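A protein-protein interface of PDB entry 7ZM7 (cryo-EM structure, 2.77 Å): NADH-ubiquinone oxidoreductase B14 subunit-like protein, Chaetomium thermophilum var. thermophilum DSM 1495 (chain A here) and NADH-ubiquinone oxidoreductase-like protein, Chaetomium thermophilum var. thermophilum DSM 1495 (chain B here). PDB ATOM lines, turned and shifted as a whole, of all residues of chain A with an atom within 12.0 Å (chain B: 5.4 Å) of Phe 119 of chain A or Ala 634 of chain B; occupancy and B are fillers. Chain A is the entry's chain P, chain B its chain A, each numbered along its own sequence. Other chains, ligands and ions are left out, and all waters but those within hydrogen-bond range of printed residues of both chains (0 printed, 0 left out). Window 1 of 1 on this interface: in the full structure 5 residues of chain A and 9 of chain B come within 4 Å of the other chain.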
ATOM      1  N   LYS A 109     -22.676 -14.006 -16.030  1.00  0.00           N
ATOM      2  CA  LYS A 109     -21.860 -14.705 -17.016  1.00  0.00           C
ATOM      3  C   LYS A 109     -20.611 -13.871 -17.258  1.00  0.00           C
ATOM      4  O   LYS A 109     -20.606 -12.963 -18.092  1.00  0.00           O
ATOM      5  CB  LYS A 109     -22.658 -14.930 -18.295  1.00  0.00           C
ATOM      6  CG  LYS A 109     -21.905 -15.629 -19.412  1.00  0.00           C
ATOM      7  CD  LYS A 109     -21.539 -14.653 -20.520  1.00  0.00           C
ATOM      8  CE  LYS A 109     -22.784 -14.022 -21.120  1.00  0.00           C
ATOM      9  NZ  LYS A 109     -22.456 -13.028 -22.176  1.00  0.00           N
ATOM     10  N   ARG A 110     -19.548 -14.166 -16.512  1.00  0.00           N
ATOM     11  CA  ARG A 110     -18.296 -13.444 -16.665  1.00  0.00           C
ATOM     12  C   ARG A 110     -17.082 -14.330 -16.863  1.00  0.00           C
ATOM     13  O   ARG A 110     -16.058 -13.834 -17.348  1.00  0.00           O
ATOM     14  CB  ARG A 110     -18.049 -12.519 -15.470  1.00  0.00           C
ATOM     15  CG  ARG A 110     -18.534 -11.119 -15.737  1.00  0.00           C
ATOM     16  CD  ARG A 110     -18.140 -10.208 -14.636  1.00  0.00           C
ATOM     17  NE  ARG A 110     -19.041 -10.315 -13.504  1.00  0.00           N
ATOM     18  CZ  ARG A 110     -18.690 -10.041 -12.262  1.00  0.00           C
ATOM     19  NH1 ARG A 110     -17.458  -9.648 -11.994  1.00  0.00           N
ATOM     20  NH2 ARG A 110     -19.577 -10.153 -11.294  1.00  0.00           N
ATOM     21  N   LEU A 111     -17.145 -15.571 -16.501  1.00  0.00           N
ATOM     22  CA  LEU A 111     -16.185 -16.518 -17.014  1.00  0.00           C
ATOM     23  C   LEU A 111     -16.725 -17.136 -18.291  1.00  0.00           C
ATOM     24  O   LEU A 111     -17.937 -17.184 -18.494  1.00  0.00           O
ATOM     25  CB  LEU A 111     -15.907 -17.626 -15.998  1.00  0.00           C
ATOM     26  CG  LEU A 111     -15.003 -17.327 -14.803  1.00  0.00           C
ATOM     27  CD1 LEU A 111     -14.626 -18.605 -14.109  1.00  0.00           C
ATOM     28  CD2 LEU A 111     -13.770 -16.580 -15.228  1.00  0.00           C
ATOM     29  N   PRO A 112     -15.865 -17.600 -19.187  1.00  0.00           N
ATOM     30  CA  PRO A 112     -16.355 -18.333 -20.354  1.00  0.00           C
ATOM     31  C   PRO A 112     -16.997 -19.652 -19.946  1.00  0.00           C
ATOM     32  O   PRO A 112     -16.588 -20.292 -18.977  1.00  0.00           O
ATOM     33  CB  PRO A 112     -15.089 -18.547 -21.184  1.00  0.00           C
ATOM     34  CG  PRO A 112     -14.005 -18.433 -20.239  1.00  0.00           C
ATOM     35  CD  PRO A 112     -14.406 -17.457 -19.209  1.00  0.00           C
ATOM     36  N   SER A 113     -18.015 -20.057 -20.705  1.00  0.00           N
ATOM     37  CA  SER A 113     -18.813 -21.217 -20.326  1.00  0.00           C
ATOM     38  C   SER A 113     -18.042 -22.515 -20.498  1.00  0.00           C
ATOM     39  O   SER A 113     -18.119 -23.413 -19.652  1.00  0.00           O
ATOM     40  CB  SER A 113     -20.095 -21.260 -21.149  1.00  0.00           C
ATOM     41  OG  SER A 113     -20.622 -22.574 -21.186  1.00  0.00           O
ATOM     42  N   ASN A 114     -17.309 -22.636 -21.592  1.00  0.00           N
ATOM     43  CA  ASN A 114     -16.586 -23.840 -21.916  1.00  0.00           C
ATOM     44  C   ASN A 114     -15.335 -23.419 -22.671  1.00  0.00           C
ATOM     45  O   ASN A 114     -14.991 -22.236 -22.708  1.00  0.00           O
ATOM     46  CB  ASN A 114     -17.493 -24.780 -22.711  1.00  0.00           C
ATOM     47  CG  ASN A 114     -17.846 -24.228 -24.062  1.00  0.00           C
ATOM     48  OD1 ASN A 114     -18.543 -23.229 -24.178  1.00  0.00           O
ATOM     49  ND2 ASN A 114     -17.342 -24.874 -25.101  1.00  0.00           N
ATOM     50  N   PHE A 115     -14.650 -24.374 -23.291  1.00  0.00           N
ATOM     51  CA  PHE A 115     -13.440 -24.003 -24.009  1.00  0.00           C
ATOM     52  C   PHE A 115     -13.745 -23.116 -25.211  1.00  0.00           C
ATOM     53  O   PHE A 115     -13.147 -22.051 -25.364  1.00  0.00           O
ATOM     54  CB  PHE A 115     -12.656 -25.234 -24.444  1.00  0.00           C
ATOM     55  CG  PHE A 115     -11.414 -24.895 -25.174  1.00  0.00           C
ATOM     56  CD1 PHE A 115     -10.257 -24.615 -24.485  1.00  0.00           C
ATOM     57  CD2 PHE A 115     -11.407 -24.798 -26.553  1.00  0.00           C
ATOM     58  CE1 PHE A 115      -9.121 -24.270 -25.154  1.00  0.00           C
ATOM     59  CE2 PHE A 115     -10.276 -24.437 -27.222  1.00  0.00           C
ATOM     60  CZ  PHE A 115      -9.133 -24.180 -26.523  1.00  0.00           C
ATOM     61  N   ILE A 116     -14.671 -23.527 -26.078  1.00  0.00           N
ATOM     62  CA  ILE A 116     -14.761 -22.899 -27.397  1.00  0.00           C
ATOM     63  C   ILE A 116     -15.287 -21.471 -27.302  1.00  0.00           C
ATOM     64  O   ILE A 116     -14.835 -20.588 -28.035  1.00  0.00           O
ATOM     65  CB  ILE A 116     -15.603 -23.755 -28.362  1.00  0.00           C
ATOM     66  CG1 ILE A 116     -15.355 -23.317 -29.798  1.00  0.00           C
ATOM     67  CG2 ILE A 116     -17.073 -23.622 -28.085  1.00  0.00           C
ATOM     68  CD1 ILE A 116     -13.957 -23.549 -30.270  1.00  0.00           C
ATOM     69  N   THR A 117     -16.247 -21.212 -26.416  1.00  0.00           N
ATOM     70  CA  THR A 117     -16.812 -19.872 -26.353  1.00  0.00           C
ATOM     71  C   THR A 117     -15.822 -18.874 -25.778  1.00  0.00           C
ATOM     72  O   THR A 117     -15.843 -17.697 -26.152  1.00  0.00           O
ATOM     73  CB  THR A 117     -18.104 -19.873 -25.548  1.00  0.00           C
ATOM     74  OG1 THR A 117     -17.846 -20.300 -24.207  1.00  0.00           O
ATOM     75  CG2 THR A 117     -19.125 -20.785 -26.193  1.00  0.00           C
ATOM     76  N   GLY A 118     -14.958 -19.314 -24.870  1.00  0.00           N
ATOM     77  CA  GLY A 118     -13.892 -18.456 -24.403  1.00  0.00           C
ATOM     78  C   GLY A 118     -12.758 -18.311 -25.383  1.00  0.00           C
ATOM     79  O   GLY A 118     -12.014 -17.332 -25.325  1.00  0.00           O
ATOM     80  N   PHE A 119     -12.593 -19.276 -26.279  1.00  0.00           N
ATOM     81  CA  PHE A 119     -11.594 -19.130 -27.326  1.00  0.00           C
ATOM     82  C   PHE A 119     -12.035 -18.106 -28.359  1.00  0.00           C
ATOM     83  O   PHE A 119     -11.220 -17.320 -28.850  1.00  0.00           O
ATOM     84  CB  PHE A 119     -11.321 -20.479 -27.984  1.00  0.00           C
ATOM     85  CG  PHE A 119     -10.355 -20.407 -29.119  1.00  0.00           C
ATOM     86  CD1 PHE A 119      -9.003 -20.479 -28.893  1.00  0.00           C
ATOM     87  CD2 PHE A 119     -10.799 -20.251 -30.411  1.00  0.00           C
ATOM     88  CE1 PHE A 119      -8.124 -20.403 -29.919  1.00  0.00           C
ATOM     89  CE2 PHE A 119      -9.906 -20.172 -31.439  1.00  0.00           C
ATOM     90  CZ  PHE A 119      -8.567 -20.247 -31.185  1.00  0.00           C
ATOM     91  N   LEU A 120     -13.311 -18.122 -28.731  1.00  0.00           N
ATOM     92  CA  LEU A 120     -13.746 -17.208 -29.822  1.00  0.00           C
ATOM     93  C   LEU A 120     -13.819 -15.771 -29.303  1.00  0.00           C
ATOM     94  O   LEU A 120     -13.764 -14.854 -30.126  1.00  0.00           O
ATOM     95  CB  LEU A 120     -15.074 -17.698 -30.402  1.00  0.00           C
ATOM     96  CG  LEU A 120     -15.018 -19.066 -31.075  1.00  0.00           C
ATOM     97  CD1 LEU A 120     -16.396 -19.503 -31.536  1.00  0.00           C
ATOM     98  CD2 LEU A 120     -14.041 -19.054 -32.238  1.00  0.00           C
ATOM     99  N   GLU A 121     -13.867 -15.589 -27.983  1.00  0.00           N
ATOM    100  CA  GLU A 121     -13.949 -14.243 -27.355  1.00  0.00           C
ATOM    101  C   GLU A 121     -12.603 -13.805 -26.772  1.00  0.00           C
ATOM    102  O   GLU A 121     -12.591 -12.752 -26.110  1.00  0.00           O
ATOM    103  CB  GLU A 121     -14.994 -14.277 -26.242  1.00  0.00           C
ATOM    104  CG  GLU A 121     -16.385 -14.616 -26.742  1.00  0.00           C
ATOM    105  CD  GLU A 121     -17.446 -14.721 -25.662  1.00  0.00           C
ATOM    106  OE1 GLU A 121     -17.081 -14.678 -24.472  1.00  0.00           O
ATOM    107  OE2 GLU A 121     -18.635 -14.845 -26.015  1.00  0.00           O
ATOM    108  N   GLY A 122     -11.533 -14.583 -26.949  1.00  0.00           N
ATOM    109  CA  GLY A 122     -10.214 -14.253 -26.357  1.00  0.00           C
ATOM    110  C   GLY A 122     -10.192 -14.349 -24.838  1.00  0.00           C
ATOM    111  O   GLY A 122      -9.964 -13.309 -24.199  1.00  0.00           O
ATOM    112  N   ARG A 123     -10.397 -15.537 -24.272  1.00  0.00           N
ATOM    113  CA  ARG A 123     -10.445 -15.769 -22.798  1.00  0.00           C
ATOM    114  C   ARG A 123     -11.548 -14.939 -22.121  1.00  0.00           C
ATOM    115  O   ARG A 123     -11.273 -14.471 -21.000  1.00  0.00           O
ATOM    116  CB  ARG A 123      -9.057 -15.640 -22.163  1.00  0.00           C
ATOM    117  CG  ARG A 123      -8.805 -16.610 -21.018  1.00  0.00           C
ATOM    118  CD  ARG A 123      -7.414 -16.585 -20.414  1.00  0.00           C
ATOM    119  NE  ARG A 123      -7.100 -15.379 -19.659  1.00  0.00           N
ATOM    120  CZ  ARG A 123      -6.272 -14.427 -20.070  1.00  0.00           C
ATOM    121  NH1 ARG A 123      -5.658 -14.539 -21.233  1.00  0.00           N
ATOM    122  NH2 ARG A 123      -6.051 -13.372 -19.309  1.00  0.00           N
ATOM    123  N   ASN A 124     -12.725 -14.785 -22.744  1.00  0.00           N
ATOM    124  CA  ASN A 124     -13.870 -13.981 -22.206  1.00  0.00           C
ATOM    125  C   ASN A 124     -13.767 -12.498 -22.595  1.00  0.00           C
ATOM    126  O   ASN A 124     -14.803 -11.851 -22.706  1.00  0.00           O
ATOM    127  CB  ASN A 124     -14.220 -14.190 -20.726  1.00  0.00           C
ATOM    128  CG  ASN A 124     -15.678 -13.890 -20.458  1.00  0.00           C
ATOM    129  OD1 ASN A 124     -16.017 -12.820 -19.961  1.00  0.00           O
ATOM    130  ND2 ASN A 124     -16.552 -14.812 -20.822  1.00  0.00           N
ATOM    131  OXT ASN A 124     -12.646 -12.027 -22.792  1.00  0.00           O
ATOM    132  N   TRP B 329     -12.072 -15.404 -35.996  1.00  0.00           N
ATOM    133  CA  TRP B 329     -11.735 -16.781 -35.667  1.00  0.00           C
ATOM    134  C   TRP B 329     -12.913 -17.708 -35.925  1.00  0.00           C
ATOM    135  O   TRP B 329     -12.727 -18.808 -36.451  1.00  0.00           O
ATOM    136  CB  TRP B 329     -11.282 -16.886 -34.213  1.00  0.00           C
ATOM    137  CG  TRP B 329      -9.844 -16.577 -34.001  1.00  0.00           C
ATOM    138  CD1 TRP B 329      -9.330 -15.434 -33.492  1.00  0.00           C
ATOM    139  CD2 TRP B 329      -8.726 -17.428 -34.284  1.00  0.00           C
ATOM    140  NE1 TRP B 329      -7.970 -15.507 -33.449  1.00  0.00           N
ATOM    141  CE2 TRP B 329      -7.574 -16.725 -33.928  1.00  0.00           C
ATOM    142  CE3 TRP B 329      -8.596 -18.718 -34.803  1.00  0.00           C
ATOM    143  CZ2 TRP B 329      -6.302 -17.264 -34.077  1.00  0.00           C
ATOM    144  CZ3 TRP B 329      -7.346 -19.241 -34.957  1.00  0.00           C
ATOM    145  CH2 TRP B 329      -6.213 -18.522 -34.600  1.00  0.00           C
ATOM    146  N   LEU B 333     -12.033 -20.651 -38.749  1.00  0.00           N
ATOM    147  CA  LEU B 333     -12.109 -22.036 -38.325  1.00  0.00           C
ATOM    148  C   LEU B 333     -13.273 -22.746 -38.986  1.00  0.00           C
ATOM    149  O   LEU B 333     -13.243 -23.967 -39.161  1.00  0.00           O
ATOM    150  CB  LEU B 333     -12.241 -22.102 -36.812  1.00  0.00           C
ATOM    151  CG  LEU B 333     -11.028 -21.705 -35.993  1.00  0.00           C
ATOM    152  CD1 LEU B 333     -11.311 -21.998 -34.550  1.00  0.00           C
ATOM    153  CD2 LEU B 333      -9.828 -22.474 -36.477  1.00  0.00           C
ATOM    154  N   ARG B 626      -3.403 -16.449 -30.924  1.00  0.00           N
ATOM    155  CA  ARG B 626      -3.874 -17.394 -29.931  1.00  0.00           C
ATOM    156  C   ARG B 626      -2.754 -18.364 -29.625  1.00  0.00           C
ATOM    157  O   ARG B 626      -1.858 -18.570 -30.438  1.00  0.00           O
ATOM    158  CB  ARG B 626      -5.118 -18.160 -30.406  1.00  0.00           C
ATOM    159  CG  ARG B 626      -6.344 -17.316 -30.610  1.00  0.00           C
ATOM    160  CD  ARG B 626      -6.935 -16.918 -29.303  1.00  0.00           C
ATOM    161  NE  ARG B 626      -8.281 -16.398 -29.444  1.00  0.00           N
ATOM    162  CZ  ARG B 626      -8.579 -15.150 -29.776  1.00  0.00           C
ATOM    163  NH1 ARG B 626      -7.629 -14.275 -30.028  1.00  0.00           N
ATOM    164  NH2 ARG B 626      -9.840 -14.790 -29.870  1.00  0.00           N
ATOM    165  N   THR B 627      -2.797 -18.940 -28.433  1.00  0.00           N
ATOM    166  CA  THR B 627      -1.834 -19.969 -28.077  1.00  0.00           C
ATOM    167  C   THR B 627      -1.940 -21.136 -29.052  1.00  0.00           C
ATOM    168  O   THR B 627      -3.034 -21.534 -29.445  1.00  0.00           O
ATOM    169  CB  THR B 627      -2.078 -20.441 -26.650  1.00  0.00           C
ATOM    170  OG1 THR B 627      -2.217 -19.307 -25.795  1.00  0.00           O
ATOM    171  CG2 THR B 627      -0.936 -21.268 -26.167  1.00  0.00           C
ATOM    172  N   TRP B 629      -1.280 -24.500 -29.102  1.00  0.00           N
ATOM    173  CA  TRP B 629      -2.012 -25.717 -28.770  1.00  0.00           C
ATOM    174  C   TRP B 629      -3.510 -25.468 -28.687  1.00  0.00           C
ATOM    175  O   TRP B 629      -4.296 -26.381 -28.941  1.00  0.00           O
ATOM    176  CB  TRP B 629      -1.501 -26.324 -27.457  1.00  0.00           C
ATOM    177  CG  TRP B 629      -2.011 -25.672 -26.197  1.00  0.00           C
ATOM    178  CD1 TRP B 629      -1.377 -24.725 -25.466  1.00  0.00           C
ATOM    179  CD2 TRP B 629      -3.255 -25.926 -25.529  1.00  0.00           C
ATOM    180  NE1 TRP B 629      -2.136 -24.367 -24.391  1.00  0.00           N
ATOM    181  CE2 TRP B 629      -3.299 -25.086 -24.407  1.00  0.00           C
ATOM    182  CE3 TRP B 629      -4.333 -26.778 -25.773  1.00  0.00           C
ATOM    183  CZ2 TRP B 629      -4.375 -25.071 -23.529  1.00  0.00           C
ATOM    184  CZ3 TRP B 629      -5.398 -26.763 -24.902  1.00  0.00           C
ATOM    185  CH2 TRP B 629      -5.415 -25.913 -23.795  1.00  0.00           C
ATOM    186  N   LYS B 630      -3.927 -24.245 -28.350  1.00  0.00           N
ATOM    187  CA  LYS B 630      -5.351 -23.938 -28.312  1.00  0.00           C
ATOM    188  C   LYS B 630      -5.965 -23.790 -29.699  1.00  0.00           C
ATOM    189  O   LYS B 630      -7.169 -23.993 -29.852  1.00  0.00           O
ATOM    190  CB  LYS B 630      -5.609 -22.676 -27.500  1.00  0.00           C
ATOM    191  CG  LYS B 630      -5.346 -22.792 -26.025  1.00  0.00           C
ATOM    192  CD  LYS B 630      -5.681 -21.490 -25.371  1.00  0.00           C
ATOM    193  CE  LYS B 630      -5.440 -21.496 -23.903  1.00  0.00           C
ATOM    194  NZ  LYS B 630      -5.792 -20.160 -23.352  1.00  0.00           N
ATOM    195  N   ILE B 631      -5.190 -23.393 -30.706  1.00  0.00           N
ATOM    196  CA  ILE B 631      -5.741 -23.359 -32.055  1.00  0.00           C
ATOM    197  C   ILE B 631      -6.094 -24.767 -32.504  1.00  0.00           C
ATOM    198  O   ILE B 631      -7.134 -24.998 -33.125  1.00  0.00           O
ATOM    199  CB  ILE B 631      -4.770 -22.673 -33.031  1.00  0.00           C
ATOM    200  CG1 ILE B 631      -4.485 -21.236 -32.580  1.00  0.00           C
ATOM    201  CG2 ILE B 631      -5.348 -22.652 -34.420  1.00  0.00           C
ATOM    202  CD1 ILE B 631      -3.329 -20.583 -33.281  1.00  0.00           C
ATOM    203  N   ILE B 632      -5.243 -25.731 -32.177  1.00  0.00           N
ATOM    204  CA  ILE B 632      -5.533 -27.120 -32.506  1.00  0.00           C
ATOM    205  C   ILE B 632      -6.765 -27.604 -31.757  1.00  0.00           C
ATOM    206  O   ILE B 632      -7.622 -28.286 -32.320  1.00  0.00           O
ATOM    207  CB  ILE B 632      -4.309 -27.996 -32.202  1.00  0.00           C
ATOM    208  CG1 ILE B 632      -3.095 -27.460 -32.963  1.00  0.00           C
ATOM    209  CG2 ILE B 632      -4.613 -29.433 -32.549  1.00  0.00           C
ATOM    210  CD1 ILE B 632      -1.781 -27.592 -32.226  1.00  0.00           C
ATOM    211  N   ARG B 633      -6.870 -27.269 -30.477  1.00  0.00           N
ATOM    212  CA  ARG B 633      -7.948 -27.796 -29.653  1.00  0.00           C
ATOM    213  C   ARG B 633      -9.296 -27.245 -30.078  1.00  0.00           C
ATOM    214  O   ARG B 633     -10.314 -27.921 -29.940  1.00  0.00           O
ATOM    215  CB  ARG B 633      -7.657 -27.488 -28.185  1.00  0.00           C
ATOM    216  CG  ARG B 633      -8.839 -27.557 -27.256  1.00  0.00           C
ATOM    217  CD  ARG B 633      -9.269 -28.972 -26.997  1.00  0.00           C
ATOM    218  NE  ARG B 633     -10.416 -29.034 -26.103  1.00  0.00           N
ATOM    219  CZ  ARG B 633     -11.666 -28.799 -26.477  1.00  0.00           C
ATOM    220  NH1 ARG B 633     -11.942 -28.477 -27.726  1.00  0.00           N
ATOM    221  NH2 ARG B 633     -12.641 -28.884 -25.596  1.00  0.00           N
ATOM    222  N   ALA B 634      -9.322 -26.020 -30.586  1.00  0.00           N
ATOM    223  CA  ALA B 634     -10.561 -25.415 -31.053  1.00  0.00           C
ATOM    224  C   ALA B 634     -11.002 -25.987 -32.397  1.00  0.00           C
ATOM    225  O   ALA B 634     -12.188 -26.258 -32.597  1.00  0.00           O
ATOM    226  CB  ALA B 634     -10.383 -23.903 -31.144  1.00  0.00           C
ATOM    227  N   VAL B 635     -10.069 -26.176 -33.334  1.00  0.00           N
ATOM    228  CA  VAL B 635     -10.422 -26.745 -34.626  1.00  0.00           C
ATOM    229  C   VAL B 635     -10.834 -28.204 -34.458  1.00  0.00           C
ATOM    230  O   VAL B 635     -11.279 -28.848 -35.411  1.00  0.00           O
ATOM    231  CB  VAL B 635      -9.248 -26.587 -35.618  1.00  0.00           C
ATOM    232  CG1 VAL B 635      -8.078 -27.435 -35.214  1.00  0.00           C
ATOM    233  CG2 VAL B 635      -9.668 -26.832 -37.056  1.00  0.00           C
ATOM    234  N   SER B 636     -10.677 -28.747 -33.256  1.00  0.00           N
ATOM    235  CA  SER B 636     -11.247 -30.044 -32.935  1.00  0.00           C
ATOM    236  C   SER B 636     -12.763 -29.971 -32.755  1.00  0.00           C
ATOM    237  O   SER B 636     -13.474 -30.925 -33.077  1.00  0.00           O
ATOM    238  CB  SER B 636     -10.573 -30.589 -31.686  1.00  0.00           C
ATOM    239  OG  SER B 636      -9.181 -30.531 -31.836  1.00  0.00           O
ATOM    240  N   GLU B 637     -13.271 -28.877 -32.191  1.00  0.00           N
ATOM    241  CA  GLU B 637     -14.716 -28.683 -32.139  1.00  0.00           C
ATOM    242  C   GLU B 637     -15.305 -28.499 -33.526  1.00  0.00           C
ATOM    243  O   GLU B 637     -16.373 -29.038 -33.829  1.00  0.00           O
ATOM    244  CB  GLU B 637     -15.075 -27.485 -31.265  1.00  0.00           C
ATOM    245  CG  GLU B 637     -14.773 -27.630 -29.801  1.00  0.00           C
ATOM    246  CD  GLU B 637     -15.642 -28.690 -29.160  1.00  0.00           C
ATOM    247  OE1 GLU B 637     -16.792 -28.867 -29.614  1.00  0.00           O
ATOM    248  OE2 GLU B 637     -15.198 -29.327 -28.185  1.00  0.00           O
ATOM    249  N   PHE B 638     -14.629 -27.737 -34.377  1.00  0.00           N
ATOM    250  CA  PHE B 638     -15.182 -27.436 -35.685  1.00  0.00           C
ATOM    251  C   PHE B 638     -15.131 -28.627 -36.627  1.00  0.00           C
ATOM    252  O   PHE B 638     -15.947 -28.702 -37.549  1.00  0.00           O
ATOM    253  CB  PHE B 638     -14.458 -26.237 -36.280  1.00  0.00           C
ATOM    254  CG  PHE B 638     -14.985 -24.932 -35.779  1.00  0.00           C
ATOM    255  CD1 PHE B 638     -14.790 -24.562 -34.470  1.00  0.00           C
ATOM    256  CD2 PHE B 638     -15.710 -24.100 -36.600  1.00  0.00           C
ATOM    257  CE1 PHE B 638     -15.284 -23.401 -33.999  1.00  0.00           C
ATOM    258  CE2 PHE B 638     -16.201 -22.921 -36.121  1.00  0.00           C
ATOM    259  CZ  PHE B 638     -15.985 -22.576 -34.817  1.00  0.00           C
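The backbone carbonyl oxygen (O) of Phe 119 of chain A is in hydrogen-bond range of the guanidinium group (NH2) of Arg 626 of chain B, at 3.1 Å. The guanidinium group (NH2) of Arg 626 of chain B lies close to the backbone NH (N) of Gly 122 of chain A (3.4 Å).
Among the printed residues, merely in contact across the chains: Phe 115 of chain A with Arg 633 of chain B (3.4 Å), Ile 116 of chain A with Ala 634 of chain B (3.7 Å), Phe 119 of chain A with Lys 630 of chain B (3.7 Å), Phe 119 of chain A with Ala 634 of chain B (3.7 Å), Phe 115 of chain A with Ala 634 of chain B (3.8 Å), Phe 115 of chain A with Lys 630 of chain B (3.9 Å), Phe 119 of chain A with Leu 333 of chain B (3.9 Å), Phe 119 of chain A with Trp 329 of chain B (3.9 Å), Leu 120 of chain A with Arg 626 of chain B (3.9 Å) and Ile 116 of chain A with Phe 638 of chain B (3.96 Å).
The side-chain amide nitrogen (ND2) of Asn 114 of chain A lies close to the backbone NH (N) of Ile 116 of chain A. O of Arg 633 of chain B sits close to OG of Ser 636 of chain B. The guanidinium group of Arg 633 of chain B is in salt-bridge range of the side-chain carboxylate of Glu 637 of chain B (3.4 Å).
Of the printed residues of chain B, Phe 119 of chain A touches Trp 329 (3.9 Å), Leu 333 (3.9 Å), Arg 626 (3.1 Å), Lys 630 (3.7 Å) and Ala 634 (3.7 Å). Of chain A, only Phe 115 (3.8 Å), Ile 116 (3.7 Å) and Phe 119 (3.7 Å) come within 4 Å of Ala 634 of chain B. Printed residues of chain A within 4 Å of Trp 329 of chain B: Phe 119 (3.9 Å). Leu 333 of chain B touches just one residue of chain A: Phe 119 (3.9 Å). Of chain A, only Phe 119 (3.1 Å), Leu 120 (3.9 Å) and Gly 122 (3.4 Å) come within 4 Å of Arg 626 of chain B. No residue of chain A comes within 4 Å of Ile 631 of chain B. Of chain A, only Phe 115 comes within 4 Å of Arg 633 of chain B. Ser 636 of chain B touches none of the printed residues of chain A. No residue of chain A comes within 4 Å of Glu 637 of chain B. Phe 638 of chain B touches just one residue of chain A: Ile 116. Printed residues of chain B within 4 Å of Leu 120 of chain A: Arg 626 (3.9 Å). Printed residues of chain B within 4 Å of Ile 116 of chain A: Ala 634 (3.7 Å) and Phe 638 (3.96 Å). Printed residues of chain B within 4 Å of Phe 115 of chain A: Lys 630, Arg 633 and Ala 634. Of the printed residues of chain B, Gly 122 of chain A touches Arg 626 (3.4 Å). Ser 113 of chain A touches none of the printed residues of chain B. The nearest residue of chain B that does not touch Phe 119 of chain A is Ile 631 of chain B (4.3 Å). The nearest printed residue of chain B that does not touch Phe 115 of chain A is Trp 629 of chain B (4.3 Å).
Of the 16 printed residues of chain A, 5 touch a printed residue of chain B. Printed residues of chain B that touch a printed residue of chain A: Trp 329, Leu 333, Arg 626, Lys 630, Arg 633, Ala 634 and Phe 638. Hydrophobic or aromatic side chains of chain B that line the printed part of chain A: Trp 329, Leu 333, Ala 634 and Phe 638. Among the printed residues, 12 pairs touch across the chains. Among the printed residues, no Asp or Glu carboxylate lies within 4 Å of a Lys or Arg side-chain nitrogen of the other chain.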
